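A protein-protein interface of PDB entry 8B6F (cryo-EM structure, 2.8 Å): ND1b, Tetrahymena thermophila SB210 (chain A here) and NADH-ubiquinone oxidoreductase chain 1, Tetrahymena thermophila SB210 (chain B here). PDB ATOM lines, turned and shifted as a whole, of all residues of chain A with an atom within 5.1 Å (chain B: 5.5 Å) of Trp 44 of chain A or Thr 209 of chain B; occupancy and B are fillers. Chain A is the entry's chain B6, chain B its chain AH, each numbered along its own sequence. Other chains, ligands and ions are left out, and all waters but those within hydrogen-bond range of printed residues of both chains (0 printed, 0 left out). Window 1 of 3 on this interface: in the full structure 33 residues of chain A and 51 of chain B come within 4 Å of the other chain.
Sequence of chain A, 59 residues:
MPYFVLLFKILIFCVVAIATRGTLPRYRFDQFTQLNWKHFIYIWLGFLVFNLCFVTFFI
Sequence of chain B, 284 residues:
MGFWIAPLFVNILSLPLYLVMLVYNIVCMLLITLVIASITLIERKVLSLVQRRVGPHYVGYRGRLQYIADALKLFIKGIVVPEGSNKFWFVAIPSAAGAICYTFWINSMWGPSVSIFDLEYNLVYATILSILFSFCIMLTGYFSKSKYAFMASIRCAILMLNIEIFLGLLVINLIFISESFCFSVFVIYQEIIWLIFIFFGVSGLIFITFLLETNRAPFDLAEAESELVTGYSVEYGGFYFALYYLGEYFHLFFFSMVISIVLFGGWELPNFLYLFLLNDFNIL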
ATOM      1  N   PHE A  40      -1.134   6.903  21.878  1.00  0.00           N
ATOM      2  CA  PHE A  40      -2.583   6.855  22.029  1.00  0.00           C
ATOM      3  C   PHE A  40      -3.111   7.954  22.939  1.00  0.00           C
ATOM      4  O   PHE A  40      -4.227   8.437  22.732  1.00  0.00           O
ATOM      5  CB  PHE A  40      -3.016   5.485  22.549  1.00  0.00           C
ATOM      6  CG  PHE A  40      -2.799   4.369  21.566  1.00  0.00           C
ATOM      7  CD1 PHE A  40      -3.073   4.553  20.220  1.00  0.00           C
ATOM      8  CD2 PHE A  40      -2.318   3.143  21.985  1.00  0.00           C
ATOM      9  CE1 PHE A  40      -2.875   3.533  19.313  1.00  0.00           C
ATOM     10  CE2 PHE A  40      -2.117   2.117  21.081  1.00  0.00           C
ATOM     11  CZ  PHE A  40      -2.396   2.314  19.743  1.00  0.00           C
ATOM     12  N   ILE A  41      -2.332   8.367  23.939  1.00  0.00           N
ATOM     13  CA  ILE A  41      -2.753   9.489  24.770  1.00  0.00           C
ATOM     14  C   ILE A  41      -2.857  10.756  23.931  1.00  0.00           C
ATOM     15  O   ILE A  41      -3.825  11.517  24.047  1.00  0.00           O
ATOM     16  CB  ILE A  41      -1.794   9.659  25.966  1.00  0.00           C
ATOM     17  CG1 ILE A  41      -2.322  10.733  26.919  1.00  0.00           C
ATOM     18  CG2 ILE A  41      -0.386  10.009  25.497  1.00  0.00           C
ATOM     19  CD1 ILE A  41      -1.600  10.787  28.247  1.00  0.00           C
ATOM     20  N   TYR A  42      -1.870  10.998  23.067  1.00  0.00           N
ATOM     21  CA  TYR A  42      -1.939  12.149  22.174  1.00  0.00           C
ATOM     22  C   TYR A  42      -3.117  12.032  21.216  1.00  0.00           C
ATOM     23  O   TYR A  42      -3.788  13.028  20.922  1.00  0.00           O
ATOM     24  CB  TYR A  42      -0.633  12.285  21.395  1.00  0.00           C
ATOM     25  CG  TYR A  42       0.588  12.471  22.263  1.00  0.00           C
ATOM     26  CD1 TYR A  42       0.938  13.722  22.752  1.00  0.00           C
ATOM     27  CD2 TYR A  42       1.400  11.392  22.581  1.00  0.00           C
ATOM     28  CE1 TYR A  42       2.062  13.892  23.540  1.00  0.00           C
ATOM     29  CE2 TYR A  42       2.522  11.549  23.367  1.00  0.00           C
ATOM     30  CZ  TYR A  42       2.848  12.800  23.843  1.00  0.00           C
ATOM     31  OH  TYR A  42       3.968  12.951  24.626  1.00  0.00           O
ATOM     32  N   ILE A  43      -3.379  10.827  20.708  1.00  0.00           N
ATOM     33  CA  ILE A  43      -4.511  10.634  19.805  1.00  0.00           C
ATOM     34  C   ILE A  43      -5.816  10.976  20.515  1.00  0.00           C
ATOM     35  O   ILE A  43      -6.681  11.666  19.962  1.00  0.00           O
ATOM     36  CB  ILE A  43      -4.525   9.192  19.262  1.00  0.00           C
ATOM     37  CG1 ILE A  43      -3.338   8.956  18.321  1.00  0.00           C
ATOM     38  CG2 ILE A  43      -5.847   8.888  18.557  1.00  0.00           C
ATOM     39  CD1 ILE A  43      -3.435   9.654  16.981  1.00  0.00           C
ATOM     40  N   TRP A  44      -5.982  10.491  21.747  1.00  0.00           N
ATOM     41  CA  TRP A  44      -7.202  10.785  22.494  1.00  0.00           C
ATOM     42  C   TRP A  44      -7.355  12.282  22.727  1.00  0.00           C
ATOM     43  O   TRP A  44      -8.439  12.845  22.536  1.00  0.00           O
ATOM     44  CB  TRP A  44      -7.194  10.047  23.830  1.00  0.00           C
ATOM     45  CG  TRP A  44      -7.541   8.593  23.754  1.00  0.00           C
ATOM     46  CD1 TRP A  44      -6.734   7.539  24.072  1.00  0.00           C
ATOM     47  CD2 TRP A  44      -8.791   8.031  23.342  1.00  0.00           C
ATOM     48  NE1 TRP A  44      -7.405   6.357  23.881  1.00  0.00           N
ATOM     49  CE2 TRP A  44      -8.670   6.632  23.433  1.00  0.00           C
ATOM     50  CE3 TRP A  44     -10.001   8.576  22.901  1.00  0.00           C
ATOM     51  CZ2 TRP A  44      -9.712   5.770  23.101  1.00  0.00           C
ATOM     52  CZ3 TRP A  44     -11.035   7.719  22.573  1.00  0.00           C
ATOM     53  CH2 TRP A  44     -10.883   6.331  22.673  1.00  0.00           C
ATOM     54  N   LEU A  45      -6.278  12.944  23.153  1.00  0.00           N
ATOM     55  CA  LEU A  45      -6.359  14.373  23.433  1.00  0.00           C
ATOM     56  C   LEU A  45      -6.640  15.168  22.168  1.00  0.00           C
ATOM     57  O   LEU A  45      -7.451  16.099  22.182  1.00  0.00           O
ATOM     58  CB  LEU A  45      -5.071  14.855  24.103  1.00  0.00           C
ATOM     59  CG  LEU A  45      -4.831  14.316  25.517  1.00  0.00           C
ATOM     60  CD1 LEU A  45      -3.458  14.719  26.022  1.00  0.00           C
ATOM     61  CD2 LEU A  45      -5.905  14.797  26.482  1.00  0.00           C
ATOM     62  N   GLY A  46      -6.003  14.801  21.057  1.00  0.00           N
ATOM     63  CA  GLY A  46      -6.290  15.474  19.803  1.00  0.00           C
ATOM     64  C   GLY A  46      -7.727  15.276  19.362  1.00  0.00           C
ATOM     65  O   GLY A  46      -8.371  16.208  18.877  1.00  0.00           O
ATOM     66  N   PHE A  47      -8.250  14.063  19.534  1.00  0.00           N
ATOM     67  CA  PHE A  47      -9.645  13.806  19.195  1.00  0.00           C
ATOM     68  C   PHE A  47     -10.580  14.634  20.065  1.00  0.00           C
ATOM     69  O   PHE A  47     -11.579  15.173  19.577  1.00  0.00           O
ATOM     70  CB  PHE A  47      -9.951  12.316  19.341  1.00  0.00           C
ATOM     71  CG  PHE A  47     -11.237  11.900  18.697  1.00  0.00           C
ATOM     72  CD1 PHE A  47     -11.274  11.558  17.357  1.00  0.00           C
ATOM     73  CD2 PHE A  47     -12.410  11.851  19.431  1.00  0.00           C
ATOM     74  CE1 PHE A  47     -12.455  11.175  16.758  1.00  0.00           C
ATOM     75  CE2 PHE A  47     -13.595  11.469  18.838  1.00  0.00           C
ATOM     76  CZ  PHE A  47     -13.617  11.130  17.501  1.00  0.00           C
ATOM     77  N   LEU A  48     -10.271  14.746  21.357  1.00  0.00           N
ATOM     78  CA  LEU A  48     -11.079  15.578  22.243  1.00  0.00           C
ATOM     79  C   LEU A  48     -11.059  17.035  21.800  1.00  0.00           C
ATOM     80  O   LEU A  48     -12.097  17.708  21.803  1.00  0.00           O
ATOM     81  CB  LEU A  48     -10.572  15.449  23.679  1.00  0.00           C
ATOM     82  CG  LEU A  48     -11.227  16.353  24.727  1.00  0.00           C
ATOM     83  CD1 LEU A  48     -12.708  16.045  24.860  1.00  0.00           C
ATOM     84  CD2 LEU A  48     -10.523  16.208  26.065  1.00  0.00           C
ATOM     85  N   VAL A  49      -9.887  17.539  21.418  1.00  0.00           N
ATOM     86  CA  VAL A  49      -9.782  18.927  20.976  1.00  0.00           C
ATOM     87  C   VAL A  49     -10.572  19.134  19.693  1.00  0.00           C
ATOM     88  O   VAL A  49     -11.243  20.159  19.518  1.00  0.00           O
ATOM     89  CB  VAL A  49      -8.304  19.313  20.804  1.00  0.00           C
ATOM     90  CG1 VAL A  49      -8.186  20.718  20.236  1.00  0.00           C
ATOM     91  CG2 VAL A  49      -7.586  19.212  22.131  1.00  0.00           C
ATOM     92  N   PHE B 166      -6.372   5.118  29.557  1.00  0.00           N
ATOM     93  CA  PHE B 166      -7.116   4.792  28.344  1.00  0.00           C
ATOM     94  C   PHE B 166      -8.614   4.950  28.568  1.00  0.00           C
ATOM     95  O   PHE B 166      -9.300   5.646  27.811  1.00  0.00           O
ATOM     96  CB  PHE B 166      -6.790   3.370  27.886  1.00  0.00           C
ATOM     97  CG  PHE B 166      -6.450   3.269  26.427  1.00  0.00           C
ATOM     98  CD1 PHE B 166      -5.150   3.457  25.991  1.00  0.00           C
ATOM     99  CD2 PHE B 166      -7.430   2.987  25.494  1.00  0.00           C
ATOM    100  CE1 PHE B 166      -4.833   3.364  24.647  1.00  0.00           C
ATOM    101  CE2 PHE B 166      -7.121   2.894  24.149  1.00  0.00           C
ATOM    102  CZ  PHE B 166      -5.821   3.083  23.725  1.00  0.00           C
ATOM    103  N   LEU B 167      -9.141   4.301  29.609  1.00  0.00           N
ATOM    104  CA  LEU B 167     -10.569   4.391  29.889  1.00  0.00           C
ATOM    105  C   LEU B 167     -10.972   5.790  30.336  1.00  0.00           C
ATOM    106  O   LEU B 167     -12.077   6.245  30.021  1.00  0.00           O
ATOM    107  CB  LEU B 167     -10.968   3.368  30.951  1.00  0.00           C
ATOM    108  CG  LEU B 167     -12.232   2.568  30.635  1.00  0.00           C
ATOM    109  CD1 LEU B 167     -12.523   1.580  31.747  1.00  0.00           C
ATOM    110  CD2 LEU B 167     -13.420   3.494  30.423  1.00  0.00           C
ATOM    111  N   LEU B 169      -9.659   8.646  29.280  1.00  0.00           N
ATOM    112  CA  LEU B 169      -9.768   9.465  28.079  1.00  0.00           C
ATOM    113  C   LEU B 169     -11.005   9.094  27.270  1.00  0.00           C
ATOM    114  O   LEU B 169     -11.680   9.973  26.724  1.00  0.00           O
ATOM    115  CB  LEU B 169      -8.497   9.327  27.246  1.00  0.00           C
ATOM    116  CG  LEU B 169      -7.248   9.888  27.932  1.00  0.00           C
ATOM    117  CD1 LEU B 169      -6.006   9.588  27.132  1.00  0.00           C
ATOM    118  CD2 LEU B 169      -7.369  11.392  28.144  1.00  0.00           C
ATOM    119  N   LEU B 170     -11.315   7.800  27.173  1.00  0.00           N
ATOM    120  CA  LEU B 170     -12.531   7.395  26.476  1.00  0.00           C
ATOM    121  C   LEU B 170     -13.761   7.985  27.152  1.00  0.00           C
ATOM    122  O   LEU B 170     -14.664   8.498  26.481  1.00  0.00           O
ATOM    123  CB  LEU B 170     -12.626   5.871  26.419  1.00  0.00           C
ATOM    124  CG  LEU B 170     -13.918   5.301  25.823  1.00  0.00           C
ATOM    125  CD1 LEU B 170     -14.187   5.871  24.439  1.00  0.00           C
ATOM    126  CD2 LEU B 170     -13.856   3.786  25.766  1.00  0.00           C
ATOM    127  N   ASN B 173     -14.038  11.737  26.487  1.00  0.00           N
ATOM    128  CA  ASN B 173     -14.595  12.021  25.169  1.00  0.00           C
ATOM    129  C   ASN B 173     -16.092  11.736  25.126  1.00  0.00           C
ATOM    130  O   ASN B 173     -16.848  12.466  24.475  1.00  0.00           O
ATOM    131  CB  ASN B 173     -13.861  11.206  24.107  1.00  0.00           C
ATOM    132  CG  ASN B 173     -12.442  11.686  23.886  1.00  0.00           C
ATOM    133  OD1 ASN B 173     -11.824  12.262  24.779  1.00  0.00           O
ATOM    134  ND2 ASN B 173     -11.916  11.451  22.691  1.00  0.00           N
ATOM    135  N   PHE B 199     -16.876   8.593  16.494  1.00  0.00           N
ATOM    136  CA  PHE B 199     -15.589   8.017  16.855  1.00  0.00           C
ATOM    137  C   PHE B 199     -15.075   7.036  15.813  1.00  0.00           C
ATOM    138  O   PHE B 199     -14.144   6.277  16.100  1.00  0.00           O
ATOM    139  CB  PHE B 199     -15.690   7.327  18.214  1.00  0.00           C
ATOM    140  CG  PHE B 199     -15.971   8.267  19.347  1.00  0.00           C
ATOM    141  CD1 PHE B 199     -17.258   8.714  19.589  1.00  0.00           C
ATOM    142  CD2 PHE B 199     -14.948   8.705  20.168  1.00  0.00           C
ATOM    143  CE1 PHE B 199     -17.519   9.582  20.632  1.00  0.00           C
ATOM    144  CE2 PHE B 199     -15.200   9.573  21.209  1.00  0.00           C
ATOM    145  CZ  PHE B 199     -16.488  10.013  21.442  1.00  0.00           C
ATOM    146  N   VAL B 202     -11.406   6.770  15.502  1.00  0.00           N
ATOM    147  CA  VAL B 202     -10.698   6.143  16.612  1.00  0.00           C
ATOM    148  C   VAL B 202     -11.332   4.791  16.910  1.00  0.00           C
ATOM    149  O   VAL B 202     -11.259   4.296  18.039  1.00  0.00           O
ATOM    150  CB  VAL B 202     -10.696   7.041  17.863  1.00  0.00           C
ATOM    151  CG1 VAL B 202      -9.979   8.349  17.572  1.00  0.00           C
ATOM    152  CG2 VAL B 202     -12.114   7.302  18.345  1.00  0.00           C
ATOM    153  N   GLY B 204     -10.311   1.954  15.984  1.00  0.00           N
ATOM    154  CA  GLY B 204      -9.246   1.075  16.433  1.00  0.00           C
ATOM    155  C   GLY B 204      -8.935   1.249  17.907  1.00  0.00           C
ATOM    156  O   GLY B 204      -8.736   0.271  18.629  1.00  0.00           O
ATOM    157  N   LEU B 205      -8.893   2.499  18.375  1.00  0.00           N
ATOM    158  CA  LEU B 205      -8.654   2.752  19.791  1.00  0.00           C
ATOM    159  C   LEU B 205      -9.810   2.257  20.652  1.00  0.00           C
ATOM    160  O   LEU B 205      -9.589   1.799  21.779  1.00  0.00           O
ATOM    161  CB  LEU B 205      -8.413   4.243  20.027  1.00  0.00           C
ATOM    162  CG  LEU B 205      -7.036   4.778  19.625  1.00  0.00           C
ATOM    163  CD1 LEU B 205      -6.849   4.782  18.115  1.00  0.00           C
ATOM    164  CD2 LEU B 205      -6.825   6.169  20.190  1.00  0.00           C
ATOM    165  N   ILE B 206     -11.042   2.346  20.150  1.00  0.00           N
ATOM    166  CA  ILE B 206     -12.185   1.812  20.886  1.00  0.00           C
ATOM    167  C   ILE B 206     -12.068   0.301  21.012  1.00  0.00           C
ATOM    168  O   ILE B 206     -12.337  -0.273  22.075  1.00  0.00           O
ATOM    169  CB  ILE B 206     -13.505   2.228  20.209  1.00  0.00           C
ATOM    170  CG1 ILE B 206     -13.763   3.715  20.434  1.00  0.00           C
ATOM    171  CG2 ILE B 206     -14.676   1.408  20.743  1.00  0.00           C
ATOM    172  CD1 ILE B 206     -14.814   4.290  19.526  1.00  0.00           C
ATOM    173  N   PHE B 207     -11.678  -0.370  19.929  1.00  0.00           N
ATOM    174  CA  PHE B 207     -11.462  -1.810  19.994  1.00  0.00           C
ATOM    175  C   PHE B 207     -10.361  -2.140  20.994  1.00  0.00           C
ATOM    176  O   PHE B 207     -10.487  -3.084  21.781  1.00  0.00           O
ATOM    177  CB  PHE B 207     -11.114  -2.337  18.600  1.00  0.00           C
ATOM    178  CG  PHE B 207     -11.531  -3.759  18.356  1.00  0.00           C
ATOM    179  CD1 PHE B 207     -11.516  -4.695  19.377  1.00  0.00           C
ATOM    180  CD2 PHE B 207     -11.939  -4.159  17.095  1.00  0.00           C
ATOM    181  CE1 PHE B 207     -11.899  -6.001  19.142  1.00  0.00           C
ATOM    182  CE2 PHE B 207     -12.322  -5.463  16.854  1.00  0.00           C
ATOM    183  CZ  PHE B 207     -12.304  -6.384  17.878  1.00  0.00           C
ATOM    184  N   ILE B 208      -9.276  -1.365  20.982  1.00  0.00           N
ATOM    185  CA  ILE B 208      -8.189  -1.579  21.933  1.00  0.00           C
ATOM    186  C   ILE B 208      -8.691  -1.409  23.359  1.00  0.00           C
ATOM    187  O   ILE B 208      -8.364  -2.203  24.248  1.00  0.00           O
ATOM    188  CB  ILE B 208      -7.020  -0.626  21.629  1.00  0.00           C
ATOM    189  CG1 ILE B 208      -6.334  -1.047  20.335  1.00  0.00           C
ATOM    190  CG2 ILE B 208      -6.018  -0.601  22.781  1.00  0.00           C
ATOM    191  CD1 ILE B 208      -5.377  -0.035  19.806  1.00  0.00           C
ATOM    192  N   THR B 209      -9.487  -0.368  23.602  1.00  0.00           N
ATOM    193  CA  THR B 209     -10.014  -0.143  24.943  1.00  0.00           C
ATOM    194  C   THR B 209     -10.901  -1.299  25.380  1.00  0.00           C
ATOM    195  O   THR B 209     -10.815  -1.760  26.524  1.00  0.00           O
ATOM    196  CB  THR B 209     -10.796   1.168  24.986  1.00  0.00           C
ATOM    197  OG1 THR B 209     -10.032   2.206  24.361  1.00  0.00           O
ATOM    198  CG2 THR B 209     -11.087   1.562  26.424  1.00  0.00           C
ATOM    199  N   PHE B 210     -11.768  -1.774  24.488  1.00  0.00           N
ATOM    200  CA  PHE B 210     -12.638  -2.892  24.829  1.00  0.00           C
ATOM    201  C   PHE B 210     -11.824  -4.124  25.208  1.00  0.00           C
ATOM    202  O   PHE B 210     -12.080  -4.760  26.235  1.00  0.00           O
ATOM    203  CB  PHE B 210     -13.568  -3.189  23.653  1.00  0.00           C
ATOM    204  CG  PHE B 210     -14.412  -4.408  23.845  1.00  0.00           C
ATOM    205  CD1 PHE B 210     -15.424  -4.423  24.788  1.00  0.00           C
ATOM    206  CD2 PHE B 210     -14.210  -5.533  23.067  1.00  0.00           C
ATOM    207  CE1 PHE B 210     -16.207  -5.543  24.962  1.00  0.00           C
ATOM    208  CE2 PHE B 210     -14.989  -6.655  23.235  1.00  0.00           C
ATOM    209  CZ  PHE B 210     -15.990  -6.661  24.184  1.00  0.00           C
ATOM    210  N   LEU B 211     -10.843  -4.483  24.379  1.00  0.00           N
ATOM    211  CA  LEU B 211     -10.035  -5.665  24.662  1.00  0.00           C
ATOM    212  C   LEU B 211      -9.223  -5.491  25.938  1.00  0.00           C
ATOM    213  O   LEU B 211      -9.107  -6.423  26.742  1.00  0.00           O
ATOM    214  CB  LEU B 211      -9.114  -5.962  23.480  1.00  0.00           C
ATOM    215  CG  LEU B 211      -9.819  -6.283  22.162  1.00  0.00           C
ATOM    216  CD1 LEU B 211      -8.801  -6.429  21.048  1.00  0.00           C
ATOM    217  CD2 LEU B 211     -10.669  -7.541  22.290  1.00  0.00           C
ATOM    218  N   LEU B 212      -8.647  -4.304  26.140  1.00  0.00           N
ATOM    219  CA  LEU B 212      -7.821  -4.073  27.321  1.00  0.00           C
ATOM    220  C   LEU B 212      -8.643  -4.170  28.598  1.00  0.00           C
ATOM    221  O   LEU B 212      -8.199  -4.763  29.588  1.00  0.00           O
ATOM    222  CB  LEU B 212      -7.147  -2.705  27.222  1.00  0.00           C
ATOM    223  CG  LEU B 212      -6.191  -2.338  28.358  1.00  0.00           C
ATOM    224  CD1 LEU B 212      -4.951  -3.217  28.357  1.00  0.00           C
ATOM    225  CD2 LEU B 212      -5.816  -0.873  28.261  1.00  0.00           C
ATOM    226  N   GLU B 213      -9.844  -3.592  28.598  1.00  0.00           N
ATOM    227  CA  GLU B 213     -10.694  -3.667  29.779  1.00  0.00           C
ATOM    228  C   GLU B 213     -11.230  -5.076  29.996  1.00  0.00           C
ATOM    229  O   GLU B 213     -11.460  -5.480  31.141  1.00  0.00           O
ATOM    230  CB  GLU B 213     -11.848  -2.676  29.654  1.00  0.00           C
ATOM    231  CG  GLU B 213     -12.697  -2.551  30.908  1.00  0.00           C
ATOM    232  CD  GLU B 213     -11.953  -1.917  32.064  1.00  0.00           C
ATOM    233  OE1 GLU B 213     -10.883  -1.319  31.830  1.00  0.00           O
ATOM    234  OE2 GLU B 213     -12.439  -2.014  33.209  1.00  0.00           O
ATOM    235  N   THR B 214     -11.443  -5.831  28.920  1.00  0.00           N
ATOM    236  CA  THR B 214     -11.914  -7.204  29.038  1.00  0.00           C
ATOM    237  C   THR B 214     -10.797  -8.187  29.362  1.00  0.00           C
ATOM    238  O   THR B 214     -11.086  -9.346  29.676  1.00  0.00           O
ATOM    239  CB  THR B 214     -12.606  -7.619  27.735  1.00  0.00           C
ATOM    240  OG1 THR B 214     -13.561  -6.619  27.358  1.00  0.00           O
ATOM    241  CG2 THR B 214     -13.327  -8.946  27.891  1.00  0.00           C
ATOM    242  N   PHE B 255     -18.870  -5.070  30.676  1.00  0.00           N
ATOM    243  CA  PHE B 255     -18.222  -4.045  29.866  1.00  0.00           C
ATOM    244  C   PHE B 255     -18.643  -4.133  28.409  1.00  0.00           C
ATOM    245  O   PHE B 255     -18.657  -3.114  27.711  1.00  0.00           O
ATOM    246  CB  PHE B 255     -16.700  -4.126  29.971  1.00  0.00           C
ATOM    247  CG  PHE B 255     -16.010  -2.883  29.485  1.00  0.00           C
ATOM    248  CD1 PHE B 255     -16.131  -1.694  30.187  1.00  0.00           C
ATOM    249  CD2 PHE B 255     -15.258  -2.894  28.323  1.00  0.00           C
ATOM    250  CE1 PHE B 255     -15.512  -0.541  29.744  1.00  0.00           C
ATOM    251  CE2 PHE B 255     -14.636  -1.741  27.875  1.00  0.00           C
ATOM    252  CZ  PHE B 255     -14.762  -0.565  28.587  1.00  0.00           C
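Phe 40 of chain A touches Phe 166 of chain B. Ile 208 of chain B touches Phe 40 of chain A (CD1 to CZ, 3.8 Å). Ile 41 of chain A touches Leu 169 of chain B. Trp 44 of chain A touches Phe 166 of chain B. Trp 44 of chain A touches Leu 169 of chain B (CB to CD1, 3.5 Å). Trp 44 of chain A touches Asn 173 of chain B (CE3 to ND2, 3.5 Å). Leu 205 of chain B touches Trp 44 of chain A (CB to CZ2, 3.7 Å). Asn 173 of chain B touches Phe 47 of chain A. CE2 of Phe 47 of chain A touches CD2 of Phe 199 of chain B, at 3.4 Å. Val 202 of chain B touches Phe 47 of chain A (CG1 to CD1, 3.5 Å).
The side-chain amide oxygen of Asn 173 of chain B lies close to the backbone carbonyl oxygen of Leu 169 of chain B, 3.0 Å away. The backbone carbonyl oxygen (O) of Leu 205 of chain B sits at hydrogen-bond distance from the side-chain hydroxyl (OG1) of Thr 209 of chain B (2.7 Å).
Of the printed residues of chain B, Ile 41 of chain A touches Leu 169. Of chain B, only Phe 166, Leu 169, Leu 170, Asn 173, Leu 205 and Thr 209 come within 4 Å of Trp 44 of chain A. Printed residues of chain A within 4 Å of Val 202 of chain B: Phe 47. Of the printed residues of chain A, Leu 205 of chain B touches Ile 43 and Trp 44. Of chain A, only Trp 44 comes within 4 Å of Thr 209 of chain B. The nearest residue of chain B that does not touch Trp 44 of chain A is Val 202 of chain B (4.4 Å). The nearest printed residue of chain B that does not touch Phe 47 of chain A is Leu 205 of chain B (6.9 Å).
Of the 10 printed residues of chain A, 6 touch a printed residue of chain B. Along chain A the printed residues that touch a printed residue of chain B span positions 40 to 48. Among the printed residues, 14 pairs touch across the chains. Among the printed residues, no Asp or Glu carboxylate lies within 4 Å of a Lys or Arg side-chain nitrogen of the other chain.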
